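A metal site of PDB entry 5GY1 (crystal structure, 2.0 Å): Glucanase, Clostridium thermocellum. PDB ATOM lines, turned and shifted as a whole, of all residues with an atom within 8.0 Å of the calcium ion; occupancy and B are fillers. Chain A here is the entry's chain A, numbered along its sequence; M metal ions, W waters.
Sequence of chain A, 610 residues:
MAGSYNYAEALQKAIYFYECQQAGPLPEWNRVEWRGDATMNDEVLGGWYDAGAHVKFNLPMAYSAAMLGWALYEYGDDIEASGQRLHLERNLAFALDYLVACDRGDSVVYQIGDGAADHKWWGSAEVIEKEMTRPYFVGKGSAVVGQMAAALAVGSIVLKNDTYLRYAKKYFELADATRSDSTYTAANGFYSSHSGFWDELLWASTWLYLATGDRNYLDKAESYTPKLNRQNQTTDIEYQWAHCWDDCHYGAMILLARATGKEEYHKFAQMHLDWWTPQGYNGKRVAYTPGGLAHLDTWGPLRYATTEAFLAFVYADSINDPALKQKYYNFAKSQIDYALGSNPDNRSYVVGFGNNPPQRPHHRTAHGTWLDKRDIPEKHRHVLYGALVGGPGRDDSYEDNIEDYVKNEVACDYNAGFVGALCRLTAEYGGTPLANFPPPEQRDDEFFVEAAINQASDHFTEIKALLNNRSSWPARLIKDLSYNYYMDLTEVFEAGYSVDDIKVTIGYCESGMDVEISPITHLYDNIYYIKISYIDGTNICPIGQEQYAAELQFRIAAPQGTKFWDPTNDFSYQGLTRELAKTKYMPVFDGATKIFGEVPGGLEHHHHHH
OG1 of Thr 568 sits at hydrogen-bond distance from OD1 of Asp 566 (2.6 Å).
OD1 of Asp 488 lies within hydrogen-bond range of OG1 of Thr 490 (2.6 Å).
Within 4 Å of the calcium ion: Asp 488, Glu 491, Asp 566, Asn 569 and Asp 570.
The calcium ion is bound by the side-chain amide oxygen (OD1) of Asn 569 (2.3 Å), the backbone carbonyl oxygen (O) of Asp 566 (2.3 Å), the backbone carbonyl oxygen (O) of Asp 488 (2.3 Å), water W1 (2.4 Å), the side-chain carboxylate (OE2) of Glu 491 (2.4 Å), the side-chain carboxylate (OD1) of Asp 570 (2.5 Å) and the side-chain carboxylate (OE1) of Glu 491 (2.7 Å).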
ATOM      1  N   THR A 461      -1.167  22.502 -36.512  1.00  0.00           N
ATOM      2  CA  THR A 461      -2.580  22.848 -36.444  1.00  0.00           C
ATOM      3  C   THR A 461      -2.732  24.240 -37.050  1.00  0.00           C
ATOM      4  O   THR A 461      -2.007  25.166 -36.682  1.00  0.00           O
ATOM      5  CB  THR A 461      -3.046  22.948 -34.978  1.00  0.00           C
ATOM      6  OG1 THR A 461      -2.954  21.665 -34.382  1.00  0.00           O
ATOM      7  CG2 THR A 461      -4.500  23.424 -34.920  1.00  0.00           C
ATOM      8  N   TYR A 486      -4.834  27.568 -26.071  1.00  0.00           N
ATOM      9  CA  TYR A 486      -4.085  26.733 -25.118  1.00  0.00           C
ATOM     10  C   TYR A 486      -3.680  25.401 -25.722  1.00  0.00           C
ATOM     11  O   TYR A 486      -4.514  24.742 -26.375  1.00  0.00           O
ATOM     12  CB  TYR A 486      -4.919  26.460 -23.864  1.00  0.00           C
ATOM     13  CG  TYR A 486      -5.251  27.690 -23.056  1.00  0.00           C
ATOM     14  CD1 TYR A 486      -4.344  28.217 -22.151  1.00  0.00           C
ATOM     15  CD2 TYR A 486      -6.486  28.331 -23.191  1.00  0.00           C
ATOM     16  CE1 TYR A 486      -4.642  29.359 -21.408  1.00  0.00           C
ATOM     17  CE2 TYR A 486      -6.802  29.452 -22.448  1.00  0.00           C
ATOM     18  CZ  TYR A 486      -5.878  29.964 -21.567  1.00  0.00           C
ATOM     19  OH  TYR A 486      -6.173  31.094 -20.831  1.00  0.00           O
ATOM     20  N   MET A 487      -2.419  25.010 -25.534  1.00  0.00           N
ATOM     21  CA  MET A 487      -1.915  23.722 -26.016  1.00  0.00           C
ATOM     22  C   MET A 487      -1.248  22.960 -24.879  1.00  0.00           C
ATOM     23  O   MET A 487      -0.824  23.557 -23.887  1.00  0.00           O
ATOM     24  CB  MET A 487      -0.828  23.894 -27.082  1.00  0.00           C
ATOM     25  CG  MET A 487      -1.096  24.813 -28.255  1.00  0.00           C
ATOM     26  SD  MET A 487       0.470  25.626 -28.696  1.00  0.00           S
ATOM     27  CE  MET A 487       0.077  27.307 -28.182  1.00  0.00           C
ATOM     28  N   ASP A 488      -1.147  21.641 -25.059  1.00  0.00           N
ATOM     29  CA  ASP A 488      -0.338  20.772 -24.209  1.00  0.00           C
ATOM     30  C   ASP A 488       0.854  20.321 -25.056  1.00  0.00           C
ATOM     31  O   ASP A 488       0.674  19.687 -26.101  1.00  0.00           O
ATOM     32  CB  ASP A 488      -1.167  19.569 -23.764  1.00  0.00           C
ATOM     33  CG  ASP A 488      -0.450  18.687 -22.744  1.00  0.00           C
ATOM     34  OD1 ASP A 488       0.809  18.696 -22.651  1.00  0.00           O
ATOM     35  OD2 ASP A 488      -1.164  17.978 -22.024  1.00  0.00           O
ATOM     36  N   LEU A 489       2.060  20.678 -24.625  1.00  0.00           N
ATOM     37  CA  LEU A 489       3.271  20.370 -25.394  1.00  0.00           C
ATOM     38  C   LEU A 489       3.982  19.116 -24.883  1.00  0.00           C
ATOM     39  O   LEU A 489       5.152  18.891 -25.183  1.00  0.00           O
ATOM     40  CB  LEU A 489       4.210  21.579 -25.407  1.00  0.00           C
ATOM     41  CG  LEU A 489       3.659  22.853 -26.071  1.00  0.00           C
ATOM     42  CD1 LEU A 489       4.711  23.952 -26.166  1.00  0.00           C
ATOM     43  CD2 LEU A 489       3.086  22.577 -27.457  1.00  0.00           C
ATOM     44  N   THR A 490       3.283  18.289 -24.098  1.00  0.00           N
ATOM     45  CA  THR A 490       3.852  17.046 -23.564  1.00  0.00           C
ATOM     46  C   THR A 490       4.501  16.226 -24.671  1.00  0.00           C
ATOM     47  O   THR A 490       5.657  15.844 -24.524  1.00  0.00           O
ATOM     48  CB  THR A 490       2.824  16.200 -22.779  1.00  0.00           C
ATOM     49  OG1 THR A 490       2.428  16.928 -21.614  1.00  0.00           O
ATOM     50  CG2 THR A 490       3.438  14.851 -22.346  1.00  0.00           C
ATOM     51  N   GLU A 491       3.813  16.025 -25.786  1.00  0.00           N
ATOM     52  CA  GLU A 491       4.369  15.211 -26.856  1.00  0.00           C
ATOM     53  C   GLU A 491       5.632  15.812 -27.498  1.00  0.00           C
ATOM     54  O   GLU A 491       6.513  15.069 -27.945  1.00  0.00           O
ATOM     55  CB  GLU A 491       3.305  14.842 -27.895  1.00  0.00           C
ATOM     56  CG  GLU A 491       2.990  15.936 -28.899  1.00  0.00           C
ATOM     57  CD  GLU A 491       1.979  16.935 -28.357  1.00  0.00           C
ATOM     58  OE1 GLU A 491       1.545  16.827 -27.194  1.00  0.00           O
ATOM     59  OE2 GLU A 491       1.579  17.810 -29.151  1.00  0.00           O
ATOM     60  N   VAL A 492       5.723  17.140 -27.514  1.00  0.00           N
ATOM     61  CA  VAL A 492       6.892  17.852 -28.027  1.00  0.00           C
ATOM     62  C   VAL A 492       8.131  17.527 -27.191  1.00  0.00           C
ATOM     63  O   VAL A 492       9.195  17.170 -27.722  1.00  0.00           O
ATOM     64  CB  VAL A 492       6.661  19.389 -28.030  1.00  0.00           C
ATOM     65  CG1 VAL A 492       7.887  20.155 -28.541  1.00  0.00           C
ATOM     66  CG2 VAL A 492       5.396  19.765 -28.822  1.00  0.00           C
ATOM     67  N   ASN A 526       3.032  21.370 -18.619  1.00  0.00           N
ATOM     68  CA  ASN A 526       3.324  21.387 -20.053  1.00  0.00           C
ATOM     69  C   ASN A 526       2.272  22.159 -20.850  1.00  0.00           C
ATOM     70  O   ASN A 526       2.102  21.943 -22.045  1.00  0.00           O
ATOM     71  CB  ASN A 526       3.495  19.968 -20.604  1.00  0.00           C
ATOM     72  CG  ASN A 526       4.680  19.239 -19.984  1.00  0.00           C
ATOM     73  OD1 ASN A 526       5.622  19.858 -19.506  1.00  0.00           O
ATOM     74  ND2 ASN A 526       4.611  17.920 -19.976  1.00  0.00           N
ATOM     75  N   PHE A 564       5.392  14.019 -34.384  1.00  0.00           N
ATOM     76  CA  PHE A 564       4.952  13.906 -32.988  1.00  0.00           C
ATOM     77  C   PHE A 564       3.770  14.812 -32.640  1.00  0.00           C
ATOM     78  O   PHE A 564       3.106  14.588 -31.628  1.00  0.00           O
ATOM     79  CB  PHE A 564       6.133  14.210 -32.062  1.00  0.00           C
ATOM     80  CG  PHE A 564       6.757  15.565 -32.280  1.00  0.00           C
ATOM     81  CD1 PHE A 564       6.140  16.717 -31.796  1.00  0.00           C
ATOM     82  CD2 PHE A 564       7.967  15.703 -32.954  1.00  0.00           C
ATOM     83  CE1 PHE A 564       6.695  17.974 -31.988  1.00  0.00           C
ATOM     84  CE2 PHE A 564       8.550  16.963 -33.139  1.00  0.00           C
ATOM     85  CZ  PHE A 564       7.914  18.093 -32.655  1.00  0.00           C
ATOM     86  N   TRP A 565       3.527  15.842 -33.450  1.00  0.00           N
ATOM     87  CA  TRP A 565       2.542  16.875 -33.111  1.00  0.00           C
ATOM     88  C   TRP A 565       1.194  16.256 -32.785  1.00  0.00           C
ATOM     89  O   TRP A 565       0.633  15.516 -33.589  1.00  0.00           O
ATOM     90  CB  TRP A 565       2.412  17.899 -34.250  1.00  0.00           C
ATOM     91  CG  TRP A 565       1.490  19.038 -33.952  1.00  0.00           C
ATOM     92  CD1 TRP A 565       0.256  19.244 -34.471  1.00  0.00           C
ATOM     93  CD2 TRP A 565       1.711  20.108 -33.020  1.00  0.00           C
ATOM     94  NE1 TRP A 565      -0.296  20.385 -33.956  1.00  0.00           N
ATOM     95  CE2 TRP A 565       0.567  20.923 -33.044  1.00  0.00           C
ATOM     96  CE3 TRP A 565       2.774  20.449 -32.178  1.00  0.00           C
ATOM     97  CZ2 TRP A 565       0.470  22.096 -32.287  1.00  0.00           C
ATOM     98  CZ3 TRP A 565       2.665  21.594 -31.406  1.00  0.00           C
ATOM     99  CH2 TRP A 565       1.522  22.400 -31.470  1.00  0.00           C
ATOM    100  N   ASP A 566       0.668  16.551 -31.605  1.00  0.00           N
ATOM    101  CA  ASP A 566      -0.590  15.956 -31.196  1.00  0.00           C
ATOM    102  C   ASP A 566      -1.542  17.036 -30.669  1.00  0.00           C
ATOM    103  O   ASP A 566      -1.453  17.447 -29.510  1.00  0.00           O
ATOM    104  CB  ASP A 566      -0.357  14.860 -30.150  1.00  0.00           C
ATOM    105  CG  ASP A 566      -1.643  14.147 -29.753  1.00  0.00           C
ATOM    106  OD1 ASP A 566      -2.714  14.426 -30.331  1.00  0.00           O
ATOM    107  OD2 ASP A 566      -1.574  13.292 -28.840  1.00  0.00           O
ATOM    108  N   PRO A 567      -2.472  17.493 -31.506  1.00  0.00           N
ATOM    109  CA  PRO A 567      -3.382  18.545 -31.056  1.00  0.00           C
ATOM    110  C   PRO A 567      -4.485  17.982 -30.156  1.00  0.00           C
ATOM    111  O   PRO A 567      -5.208  18.754 -29.525  1.00  0.00           O
ATOM    112  CB  PRO A 567      -3.979  19.047 -32.378  1.00  0.00           C
ATOM    113  CG  PRO A 567      -4.015  17.814 -33.242  1.00  0.00           C
ATOM    114  CD  PRO A 567      -2.752  17.061 -32.892  1.00  0.00           C
ATOM    115  N   THR A 568      -4.617  16.653 -30.099  1.00  0.00           N
ATOM    116  CA  THR A 568      -5.753  16.015 -29.414  1.00  0.00           C
ATOM    117  C   THR A 568      -5.678  16.183 -27.903  1.00  0.00           C
ATOM    118  O   THR A 568      -6.690  16.021 -27.223  1.00  0.00           O
ATOM    119  CB  THR A 568      -5.970  14.497 -29.738  1.00  0.00           C
ATOM    120  OG1 THR A 568      -4.937  13.722 -29.116  1.00  0.00           O
ATOM    121  CG2 THR A 568      -6.009  14.221 -31.234  1.00  0.00           C
ATOM    122  N   ASN A 569      -4.506  16.533 -27.373  1.00  0.00           N
ATOM    123  CA  ASN A 569      -4.433  16.873 -25.957  1.00  0.00           C
ATOM    124  C   ASN A 569      -4.434  18.367 -25.665  1.00  0.00           C
ATOM    125  O   ASN A 569      -4.269  18.758 -24.513  1.00  0.00           O
ATOM    126  CB  ASN A 569      -3.235  16.169 -25.276  1.00  0.00           C
ATOM    127  CG  ASN A 569      -1.897  16.543 -25.886  1.00  0.00           C
ATOM    128  OD1 ASN A 569      -1.815  17.453 -26.718  1.00  0.00           O
ATOM    129  ND2 ASN A 569      -0.846  15.837 -25.488  1.00  0.00           N
ATOM    130  N   ASP A 570      -4.630  19.203 -26.682  1.00  0.00           N
ATOM    131  CA  ASP A 570      -4.656  20.662 -26.526  1.00  0.00           C
ATOM    132  C   ASP A 570      -6.026  21.140 -26.052  1.00  0.00           C
ATOM    133  O   ASP A 570      -7.055  20.844 -26.674  1.00  0.00           O
ATOM    134  CB  ASP A 570      -4.316  21.346 -27.851  1.00  0.00           C
ATOM    135  CG  ASP A 570      -2.899  21.016 -28.315  1.00  0.00           C
ATOM    136  OD1 ASP A 570      -2.146  20.384 -27.537  1.00  0.00           O
ATOM    137  OD2 ASP A 570      -2.537  21.385 -29.453  1.00  0.00           O
ATOM    138  N   PHE A 571      -6.024  21.865 -24.949  1.00  0.00           N
ATOM    139  CA  PHE A 571      -7.247  22.410 -24.346  1.00  0.00           C
ATOM    140  C   PHE A 571      -8.143  23.130 -25.375  1.00  0.00           C
ATOM    141  O   PHE A 571      -9.343  22.881 -25.448  1.00  0.00           O
ATOM    142  CB  PHE A 571      -6.839  23.351 -23.206  1.00  0.00           C
ATOM    143  CG  PHE A 571      -7.996  24.027 -22.499  1.00  0.00           C
ATOM    144  CD1 PHE A 571      -8.612  23.410 -21.413  1.00  0.00           C
ATOM    145  CD2 PHE A 571      -8.442  25.274 -22.905  1.00  0.00           C
ATOM    146  CE1 PHE A 571      -9.663  24.029 -20.738  1.00  0.00           C
ATOM    147  CE2 PHE A 571      -9.503  25.902 -22.235  1.00  0.00           C
ATOM    148  CZ  PHE A 571     -10.100  25.287 -21.145  1.00  0.00           C
ATOM    149  N   TYR A 573      -8.230  22.860 -28.596  1.00  0.00           N
ATOM    150  CA  TYR A 573      -8.587  22.111 -29.800  1.00  0.00           C
ATOM    151  C   TYR A 573      -9.865  21.306 -29.528  1.00  0.00           C
ATOM    152  O   TYR A 573     -10.496  20.837 -30.479  1.00  0.00           O
ATOM    153  CB  TYR A 573      -7.468  21.119 -30.155  1.00  0.00           C
ATOM    154  CG  TYR A 573      -7.440  20.537 -31.561  1.00  0.00           C
ATOM    155  CD1 TYR A 573      -7.102  21.326 -32.667  1.00  0.00           C
ATOM    156  CD2 TYR A 573      -7.666  19.169 -31.774  1.00  0.00           C
ATOM    157  CE1 TYR A 573      -7.005  20.787 -33.947  1.00  0.00           C
ATOM    158  CE2 TYR A 573      -7.559  18.622 -33.050  1.00  0.00           C
ATOM    159  CZ  TYR A 573      -7.230  19.427 -34.130  1.00  0.00           C
ATOM    160  OH  TYR A 573      -7.128  18.894 -35.389  1.00  0.00           O
HETATM  161 CA    CA M   1      -0.299  18.691 -27.943  1.00  0.00          CA
HETATM  162  O   HOH W   1       0.061  20.461 -29.500  1.00  0.00           O
